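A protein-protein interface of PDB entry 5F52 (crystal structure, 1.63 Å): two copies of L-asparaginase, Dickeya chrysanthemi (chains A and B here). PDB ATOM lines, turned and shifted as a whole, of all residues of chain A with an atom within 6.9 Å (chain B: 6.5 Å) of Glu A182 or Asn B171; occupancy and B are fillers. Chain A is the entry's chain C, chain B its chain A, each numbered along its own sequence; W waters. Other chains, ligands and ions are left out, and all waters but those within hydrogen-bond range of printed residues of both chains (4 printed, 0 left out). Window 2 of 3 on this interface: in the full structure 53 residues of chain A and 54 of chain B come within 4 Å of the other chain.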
ATOM      1  N   LYS A 179       9.731   1.537 -23.936  1.00  0.00           N
ATOM      2  CA  LYS A 179      10.543   1.537 -22.715  1.00  0.00           C
ATOM      3  C   LYS A 179      11.902   0.952 -23.027  1.00  0.00           C
ATOM      4  O   LYS A 179      12.087   0.218 -24.004  1.00  0.00           O
ATOM      5  CB  LYS A 179       9.880   0.698 -21.649  1.00  0.00           C
ATOM      6  CG  LYS A 179       8.462   1.095 -21.298  1.00  0.00           C
ATOM      7  CD  LYS A 179       7.879   0.107 -20.254  1.00  0.00           C
ATOM      8  CE  LYS A 179       6.359   0.227 -20.184  1.00  0.00           C
ATOM      9  NZ  LYS A 179       5.897   1.544 -19.651  1.00  0.00           N
ATOM     10  N   ALA A 180      12.855   1.207 -22.131  1.00  0.00           N
ATOM     11  CA  ALA A 180      14.107   0.472 -22.159  1.00  0.00           C
ATOM     12  C   ALA A 180      14.296   0.052 -20.709  1.00  0.00           C
ATOM     13  O   ALA A 180      14.797   0.818 -19.888  1.00  0.00           O
ATOM     14  CB  ALA A 180      15.177   1.378 -22.575  1.00  0.00           C
ATOM     15  N   ASN A 181      13.931  -1.172 -20.391  1.00  0.00           N
ATOM     16  CA  ASN A 181      13.858  -1.551 -18.993  1.00  0.00           C
ATOM     17  C   ASN A 181      15.170  -1.436 -18.235  1.00  0.00           C
ATOM     18  O   ASN A 181      15.202  -0.927 -17.120  1.00  0.00           O
ATOM     19  CB  ASN A 181      13.306  -2.928 -18.852  1.00  0.00           C
ATOM     20  CG  ASN A 181      11.818  -2.999 -19.323  1.00  0.00           C
ATOM     21  OD1 ASN A 181      11.004  -2.212 -18.888  1.00  0.00           O
ATOM     22  ND2 ASN A 181      11.525  -3.891 -20.286  1.00  0.00           N
ATOM     23  N   GLU A 182      16.266  -1.802 -18.844  1.00  0.00           N
ATOM     24  CA  GLU A 182      17.549  -1.773 -18.131  1.00  0.00           C
ATOM     25  C   GLU A 182      18.283  -0.466 -18.297  1.00  0.00           C
ATOM     26  O   GLU A 182      19.166  -0.178 -17.530  1.00  0.00           O
ATOM     27  CB  GLU A 182      18.406  -2.924 -18.621  1.00  0.00           C
ATOM     28  CG  GLU A 182      17.818  -4.302 -18.260  1.00  0.00           C
ATOM     29  CD  GLU A 182      17.986  -4.627 -16.761  1.00  0.00           C
ATOM     30  OE1 GLU A 182      19.160  -4.608 -16.280  1.00  0.00           O
ATOM     31  OE2 GLU A 182      16.978  -4.958 -16.066  1.00  0.00           O
ATOM     32  N   GLU A 183      18.015   0.261 -19.381  1.00  0.00           N
ATOM     33  CA  GLU A 183      18.797   1.450 -19.783  1.00  0.00           C
ATOM     34  C   GLU A 183      18.089   2.786 -19.573  1.00  0.00           C
ATOM     35  O   GLU A 183      18.737   3.834 -19.638  1.00  0.00           O
ATOM     36  CB  GLU A 183      19.266   1.376 -21.215  1.00  0.00           C
ATOM     37  CG  GLU A 183      19.994   0.059 -21.533  1.00  0.00           C
ATOM     38  CD  GLU A 183      19.140  -1.015 -22.097  1.00  0.00           C
ATOM     39  OE1 GLU A 183      17.852  -0.900 -22.060  1.00  0.00           O
ATOM     40  OE2 GLU A 183      19.751  -2.005 -22.642  1.00  0.00           O
ATOM     41  N   GLY A 184      16.817   2.739 -19.301  1.00  0.00           N
ATOM     42  CA  GLY A 184      16.061   3.940 -19.074  1.00  0.00           C
ATOM     43  C   GLY A 184      15.919   4.834 -20.289  1.00  0.00           C
ATOM     44  O   GLY A 184      16.271   4.471 -21.431  1.00  0.00           O
ATOM     45  N   GLY A 252      16.434 -17.792 -23.646  1.00  0.00           N
ATOM     46  CA  GLY A 252      17.341 -17.289 -22.638  1.00  0.00           C
ATOM     47  C   GLY A 252      18.491 -16.500 -23.214  1.00  0.00           C
ATOM     48  O   GLY A 252      18.271 -15.641 -24.080  1.00  0.00           O
ATOM     49  N   ALA A 253      19.691 -16.786 -22.728  1.00  0.00           N
ATOM     50  CA  ALA A 253      20.899 -16.072 -23.153  1.00  0.00           C
ATOM     51  C   ALA A 253      21.467 -16.648 -24.443  1.00  0.00           C
ATOM     52  O   ALA A 253      22.563 -17.089 -24.472  1.00  0.00           O
ATOM     53  CB  ALA A 253      21.886 -16.060 -22.027  1.00  0.00           C
ATOM     54  N   THR A 278      18.358 -12.811 -28.076  1.00  0.00           N
ATOM     55  CA  THR A 278      17.433 -13.389 -27.121  1.00  0.00           C
ATOM     56  C   THR A 278      16.010 -13.044 -27.406  1.00  0.00           C
ATOM     57  O   THR A 278      15.774 -11.995 -27.837  1.00  0.00           O
ATOM     58  CB  THR A 278      17.785 -12.901 -25.676  1.00  0.00           C
ATOM     59  OG1 THR A 278      16.884 -13.403 -24.725  1.00  0.00           O
ATOM     60  CG2 THR A 278      17.859 -11.372 -25.546  1.00  0.00           C
ATOM     61  N   THR A 280      13.918 -12.943 -24.999  1.00  0.00           N
ATOM     62  CA  THR A 280      13.407 -12.520 -23.710  1.00  0.00           C
ATOM     63  C   THR A 280      12.903 -11.124 -23.597  1.00  0.00           C
ATOM     64  O   THR A 280      11.989 -10.877 -22.890  1.00  0.00           O
ATOM     65  CB  THR A 280      14.437 -12.690 -22.589  1.00  0.00           C
ATOM     66  OG1 THR A 280      15.588 -11.922 -22.868  1.00  0.00           O
ATOM     67  CG2 THR A 280      14.760 -14.143 -22.421  1.00  0.00           C
ATOM     68  N   GLY A 281      13.570 -10.263 -24.308  1.00  0.00           N
ATOM     69  CA  GLY A 281      13.213  -8.887 -24.340  1.00  0.00           C
ATOM     70  C   GLY A 281      14.265  -7.921 -23.827  1.00  0.00           C
ATOM     71  O   GLY A 281      14.241  -6.787 -24.145  1.00  0.00           O
ATOM     72  N   ASN A 282      15.169  -8.431 -23.027  1.00  0.00           N
ATOM     73  CA  ASN A 282      16.167  -7.606 -22.459  1.00  0.00           C
ATOM     74  C   ASN A 282      17.411  -8.368 -22.067  1.00  0.00           C
ATOM     75  O   ASN A 282      17.409  -9.510 -21.970  1.00  0.00           O
ATOM     76  CB  ASN A 282      15.642  -7.069 -21.115  1.00  0.00           C
ATOM     77  CG  ASN A 282      14.285  -6.381 -21.200  1.00  0.00           C
ATOM     78  OD1 ASN A 282      14.233  -5.207 -21.220  1.00  0.00           O
ATOM     79  ND2 ASN A 282      13.225  -7.118 -21.181  1.00  0.00           N
ATOM     80  N   GLY A 283      18.464  -7.615 -21.820  1.00  0.00           N
ATOM     81  CA  GLY A 283      19.661  -8.178 -21.290  1.00  0.00           C
ATOM     82  C   GLY A 283      20.769  -8.571 -22.218  1.00  0.00           C
ATOM     83  O   GLY A 283      20.694  -8.413 -23.366  1.00  0.00           O
ATOM     84  N   ILE A 284      21.794  -9.104 -21.590  1.00  0.00           N
ATOM     85  CA  ILE A 284      22.997  -9.495 -22.276  1.00  0.00           C
ATOM     86  C   ILE A 284      23.121 -10.955 -22.642  1.00  0.00           C
ATOM     87  O   ILE A 284      22.953 -11.753 -21.844  1.00  0.00           O
ATOM     88  CB  ILE A 284      24.239  -9.237 -21.365  1.00  0.00           C
ATOM     89  CG1 ILE A 284      24.293  -7.784 -20.952  1.00  0.00           C
ATOM     90  CG2 ILE A 284      25.544  -9.588 -22.062  1.00  0.00           C
ATOM     91  CD1 ILE A 284      24.703  -6.865 -22.047  1.00  0.00           C
ATOM     92  N   MET B 122      19.278 -19.127 -12.108  1.00  0.00           N
ATOM     93  CA  MET B 122      20.096 -18.453 -13.076  1.00  0.00           C
ATOM     94  C   MET B 122      21.573 -18.680 -12.933  1.00  0.00           C
ATOM     95  O   MET B 122      22.296 -18.552 -13.918  1.00  0.00           O
ATOM     96  CB  MET B 122      19.743 -16.996 -13.145  1.00  0.00           C
ATOM     97  CG  MET B 122      18.312 -16.752 -13.642  1.00  0.00           C
ATOM     98  SD  MET B 122      18.199 -17.080 -15.431  1.00  0.00           S
ATOM     99  CE  MET B 122      19.102 -15.712 -16.089  1.00  0.00           C
ATOM    100  N   THR B 168       7.132 -14.915 -17.585  1.00  0.00           N
ATOM    101  CA  THR B 168       8.033 -15.148 -18.692  1.00  0.00           C
ATOM    102  C   THR B 168       9.449 -14.744 -18.260  1.00  0.00           C
ATOM    103  O   THR B 168       9.615 -13.905 -17.362  1.00  0.00           O
ATOM    104  CB  THR B 168       7.576 -14.404 -19.944  1.00  0.00           C
ATOM    105  OG1 THR B 168       8.460 -14.619 -21.043  1.00  0.00           O
ATOM    106  CG2 THR B 168       7.502 -12.906 -19.737  1.00  0.00           C
ATOM    107  N   LYS B 169      10.456 -15.338 -18.923  1.00  0.00           N
ATOM    108  CA  LYS B 169      11.819 -14.960 -18.716  1.00  0.00           C
ATOM    109  C   LYS B 169      12.023 -13.680 -19.527  1.00  0.00           C
ATOM    110  O   LYS B 169      11.949 -13.682 -20.758  1.00  0.00           O
ATOM    111  CB  LYS B 169      12.761 -16.079 -19.170  1.00  0.00           C
ATOM    112  CG  LYS B 169      14.214 -15.809 -18.882  1.00  0.00           C
ATOM    113  CD  LYS B 169      15.123 -17.035 -19.188  1.00  0.00           C
ATOM    114  CE  LYS B 169      16.544 -16.653 -18.829  1.00  0.00           C
ATOM    115  NZ  LYS B 169      17.463 -17.806 -18.928  1.00  0.00           N
ATOM    116  N   THR B 170      12.185 -12.545 -18.850  1.00  0.00           N
ATOM    117  CA  THR B 170      12.204 -11.254 -19.487  1.00  0.00           C
ATOM    118  C   THR B 170      13.611 -10.724 -19.750  1.00  0.00           C
ATOM    119  O   THR B 170      13.780  -9.754 -20.481  1.00  0.00           O
ATOM    120  CB  THR B 170      11.495 -10.167 -18.693  1.00  0.00           C
ATOM    121  OG1 THR B 170      12.191  -9.847 -17.487  1.00  0.00           O
ATOM    122  CG2 THR B 170      10.045 -10.508 -18.407  1.00  0.00           C
ATOM    123  N   ASN B 171      14.601 -11.348 -19.135  1.00  0.00           N
ATOM    124  CA  ASN B 171      15.967 -10.936 -19.284  1.00  0.00           C
ATOM    125  C   ASN B 171      16.824 -12.173 -19.536  1.00  0.00           C
ATOM    126  O   ASN B 171      16.669 -13.195 -18.898  1.00  0.00           O
ATOM    127  CB  ASN B 171      16.421 -10.198 -17.994  1.00  0.00           C
ATOM    128  CG  ASN B 171      17.770  -9.481 -18.168  1.00  0.00           C
ATOM    129  OD1 ASN B 171      18.791 -10.122 -18.342  1.00  0.00           O
ATOM    130  ND2 ASN B 171      17.776  -8.171 -18.063  1.00  0.00           N
ATOM    131  N   ALA B 172      17.771 -12.027 -20.433  1.00  0.00           N
ATOM    132  CA  ALA B 172      18.630 -13.125 -20.744  1.00  0.00           C
ATOM    133  C   ALA B 172      19.452 -13.689 -19.597  1.00  0.00           C
ATOM    134  O   ALA B 172      19.714 -14.823 -19.548  1.00  0.00           O
ATOM    135  CB  ALA B 172      19.591 -12.724 -21.852  1.00  0.00           C
ATOM    136  N   SER B 173      19.839 -12.823 -18.685  1.00  0.00           N
ATOM    137  CA  SER B 173      20.806 -13.184 -17.709  1.00  0.00           C
ATOM    138  C   SER B 173      20.733 -12.800 -16.243  1.00  0.00           C
ATOM    139  O   SER B 173      21.605 -13.145 -15.519  1.00  0.00           O
ATOM    140  CB  SER B 173      22.161 -12.670 -18.246  1.00  0.00           C
ATOM    141  OG  SER B 173      22.487 -13.206 -19.498  1.00  0.00           O
ATOM    142  N   THR B 174      19.701 -12.109 -15.823  1.00  0.00           N
ATOM    143  CA  THR B 174      19.624 -11.670 -14.427  1.00  0.00           C
ATOM    144  C   THR B 174      18.807 -12.563 -13.478  1.00  0.00           C
ATOM    145  O   THR B 174      17.992 -13.279 -13.911  1.00  0.00           O
ATOM    146  CB  THR B 174      18.984 -10.284 -14.415  1.00  0.00           C
ATOM    147  OG1 THR B 174      17.758 -10.359 -15.107  1.00  0.00           O
ATOM    148  CG2 THR B 174      19.860  -9.311 -15.106  1.00  0.00           C
ATOM    149  N   ASP B 176      16.467 -11.789 -11.468  1.00  0.00           N
ATOM    150  CA  ASP B 176      15.113 -11.315 -11.335  1.00  0.00           C
ATOM    151  C   ASP B 176      14.340 -11.361 -12.651  1.00  0.00           C
ATOM    152  O   ASP B 176      13.288 -10.758 -12.780  1.00  0.00           O
ATOM    153  CB  ASP B 176      15.102  -9.863 -10.775  1.00  0.00           C
ATOM    154  CG  ASP B 176      15.945  -8.918 -11.555  1.00  0.00           C
ATOM    155  OD1 ASP B 176      17.207  -9.071 -11.573  1.00  0.00           O
ATOM    156  OD2 ASP B 176      15.380  -7.965 -12.140  1.00  0.00           O
ATOM    157  N   THR B 177      14.868 -12.117 -13.596  1.00  0.00           N
ATOM    158  CA  THR B 177      14.345 -12.195 -14.956  1.00  0.00           C
ATOM    159  C   THR B 177      12.871 -12.602 -15.089  1.00  0.00           C
ATOM    160  O   THR B 177      12.199 -12.092 -15.979  1.00  0.00           O
ATOM    161  CB  THR B 177      15.222 -13.134 -15.732  1.00  0.00           C
ATOM    162  OG1 THR B 177      14.795 -13.204 -17.079  1.00  0.00           O
ATOM    163  CG2 THR B 177      15.209 -14.563 -15.110  1.00  0.00           C
ATOM    164  N   PHE B 178      12.354 -13.455 -14.202  1.00  0.00           N
ATOM    165  CA  PHE B 178      10.957 -13.913 -14.329  1.00  0.00           C
ATOM    166  C   PHE B 178      10.005 -12.826 -13.784  1.00  0.00           C
ATOM    167  O   PHE B 178      10.006 -12.549 -12.595  1.00  0.00           O
ATOM    168  CB  PHE B 178      10.755 -15.227 -13.664  1.00  0.00           C
ATOM    169  CG  PHE B 178      11.360 -16.324 -14.455  1.00  0.00           C
ATOM    170  CD1 PHE B 178      10.672 -16.842 -15.557  1.00  0.00           C
ATOM    171  CD2 PHE B 178      12.620 -16.730 -14.226  1.00  0.00           C
ATOM    172  CE1 PHE B 178      11.226 -17.869 -16.348  1.00  0.00           C
ATOM    173  CE2 PHE B 178      13.167 -17.796 -14.973  1.00  0.00           C
ATOM    174  CZ  PHE B 178      12.496 -18.308 -16.069  1.00  0.00           C
ATOM    175  N   LYS B 179       9.253 -12.228 -14.679  1.00  0.00           N
ATOM    176  CA  LYS B 179       8.312 -11.129 -14.348  1.00  0.00           C
ATOM    177  C   LYS B 179       7.071 -11.280 -15.226  1.00  0.00           C
ATOM    178  O   LYS B 179       7.113 -11.986 -16.245  1.00  0.00           O
ATOM    179  CB  LYS B 179       8.905  -9.780 -14.658  1.00  0.00           C
ATOM    180  CG  LYS B 179      10.203  -9.472 -13.989  1.00  0.00           C
ATOM    181  CD  LYS B 179      10.734  -8.120 -14.389  1.00  0.00           C
ATOM    182  CE  LYS B 179      12.222  -7.948 -14.062  1.00  0.00           C
ATOM    183  NZ  LYS B 179      12.483  -7.894 -12.580  1.00  0.00           N
HETATM  184  O   HOH W   1      15.376  -6.800 -17.105  1.00  0.00           O
HETATM  185  O   HOH W   2      21.389  -9.067 -18.559  1.00  0.00           O
HETATM  186  O   HOH W   3      20.453  -6.514 -18.052  1.00  0.00           O
HETATM  187  O   HOH W   4       9.569 -12.516 -22.273  1.00  0.00           O
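Of the 12 printed residues of chain B, 5 touch a printed residue of chain A. Hydrophobic or aromatic side chains of chain B within 4 Å of the printed part of chain A: Ala B172. Of the 14 printed residues of chain A, 8 touch a printed residue of chain B. Hydrophobic or aromatic side chains of chain A that line the printed part of chain B: Ala A253. Among the printed residues, 16 pairs touch across the chains. Among the printed residues, no Asp or Glu carboxylate lies within 4 Å of a Lys or Arg side-chain nitrogen of the other chain.
Water W1 bridges OE2 of Glu A182 (2.7 Å) and ND2 of Asn B171 (2.9 Å). Water W4 lies within hydrogen-bond range of OG1 of Thr B168 (2.7 Å), O of Thr A280 (3.0 Å) and O of Lys B169 (3.1 Å). Water W2 lies within hydrogen-bond range of the side-chain amide oxygen (OD1) of Asn B171 and the backbone NH (N) of Ile A284. Water W3 bridges OE1 of Glu A182 (2.9 Å) and ND2 of Asn B171 (3.1 Å).
Position printed for both chains: 179. Of the 16 pairs that touch across the chains among the printed residues, none has its exchanged pair printed and touching as well.
Of chain B, only Asn B171 comes within 4 Å of Glu A182. Of the printed residues of chain B, Ala A253 touches Ala B172 and Ser B173. Of the printed residues of chain A, Lys B169 touches Gly A252 (3.7 Å) and Thr A280 (3.2 Å). Printed residues of chain A within 4 Å of Thr B170: Thr A280, Gly A281 and Asn A282. Asn B171 touches four residues of chain A. The nearest residue of chain B that does not touch Glu A182 is Thr B174 (4.9 Å). The nearest residue of chain A that does not touch Asn B171 is Ile A284 (4.5 Å).
Among the printed residues, merely in contact across the chains: Glu A182 with Asn B171, Gly A252 with Lys B169, Gly A252 with Ala B172, Ala A253 with Ala B172, Ala A253 with Ser B173, Thr A280 with Lys B169, Thr A280 with Asn B171, Gly A281 with Thr B170, Asn A282 with Asn B171, Gly A283 with Asn B171 and Ile A284 with Ala B172.
The side-chain hydroxyl (OG1) of Thr A280 lies within hydrogen-bond range of the backbone NH (N) of Ala B172 (3.3 Å). O of Thr A280 sits close to O of Thr B170 (3.2 Å). The backbone carbonyl oxygen (O) of Asn A282 lies within hydrogen-bond range of the backbone NH (N) of Ala B172, at 3.0 Å. The backbone carbonyl oxygen (O) of Thr B170 lies within hydrogen-bond range of the side-chain amide nitrogen (ND2) of Asn A282 (2.8 Å). The side-chain hydroxyl of Ser B173 lies within hydrogen-bond range of the backbone carbonyl oxygen of Ile A284, 2.8 Å away.
The backbone carbonyl oxygen (O) of Gly A252 sits at hydrogen-bond distance from the side-chain hydroxyl (OG1) of Thr A278, at 2.7 Å. The backbone carbonyl oxygen of Thr B177 sits at hydrogen-bond distance from the side-chain hydroxyl of Thr B170 (2.7 Å). The side-chain amide oxygen of Asn A282 sits at hydrogen-bond distance from the side-chain amide nitrogen of Asn A181 (3.2 Å). The side-chain amide oxygen (OD1) of Asn B171 sits at hydrogen-bond distance from the backbone NH (N) of Ser B173 (2.9 Å). The side-chain amino group (NZ) of Lys B169 sits at hydrogen-bond distance from the side-chain sulfur (SD) of Met B122, 3.6 Å away. The side-chain hydroxyl of Thr A280 lies within hydrogen-bond range of the side-chain hydroxyl of Thr A278, 2.7 Å away.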
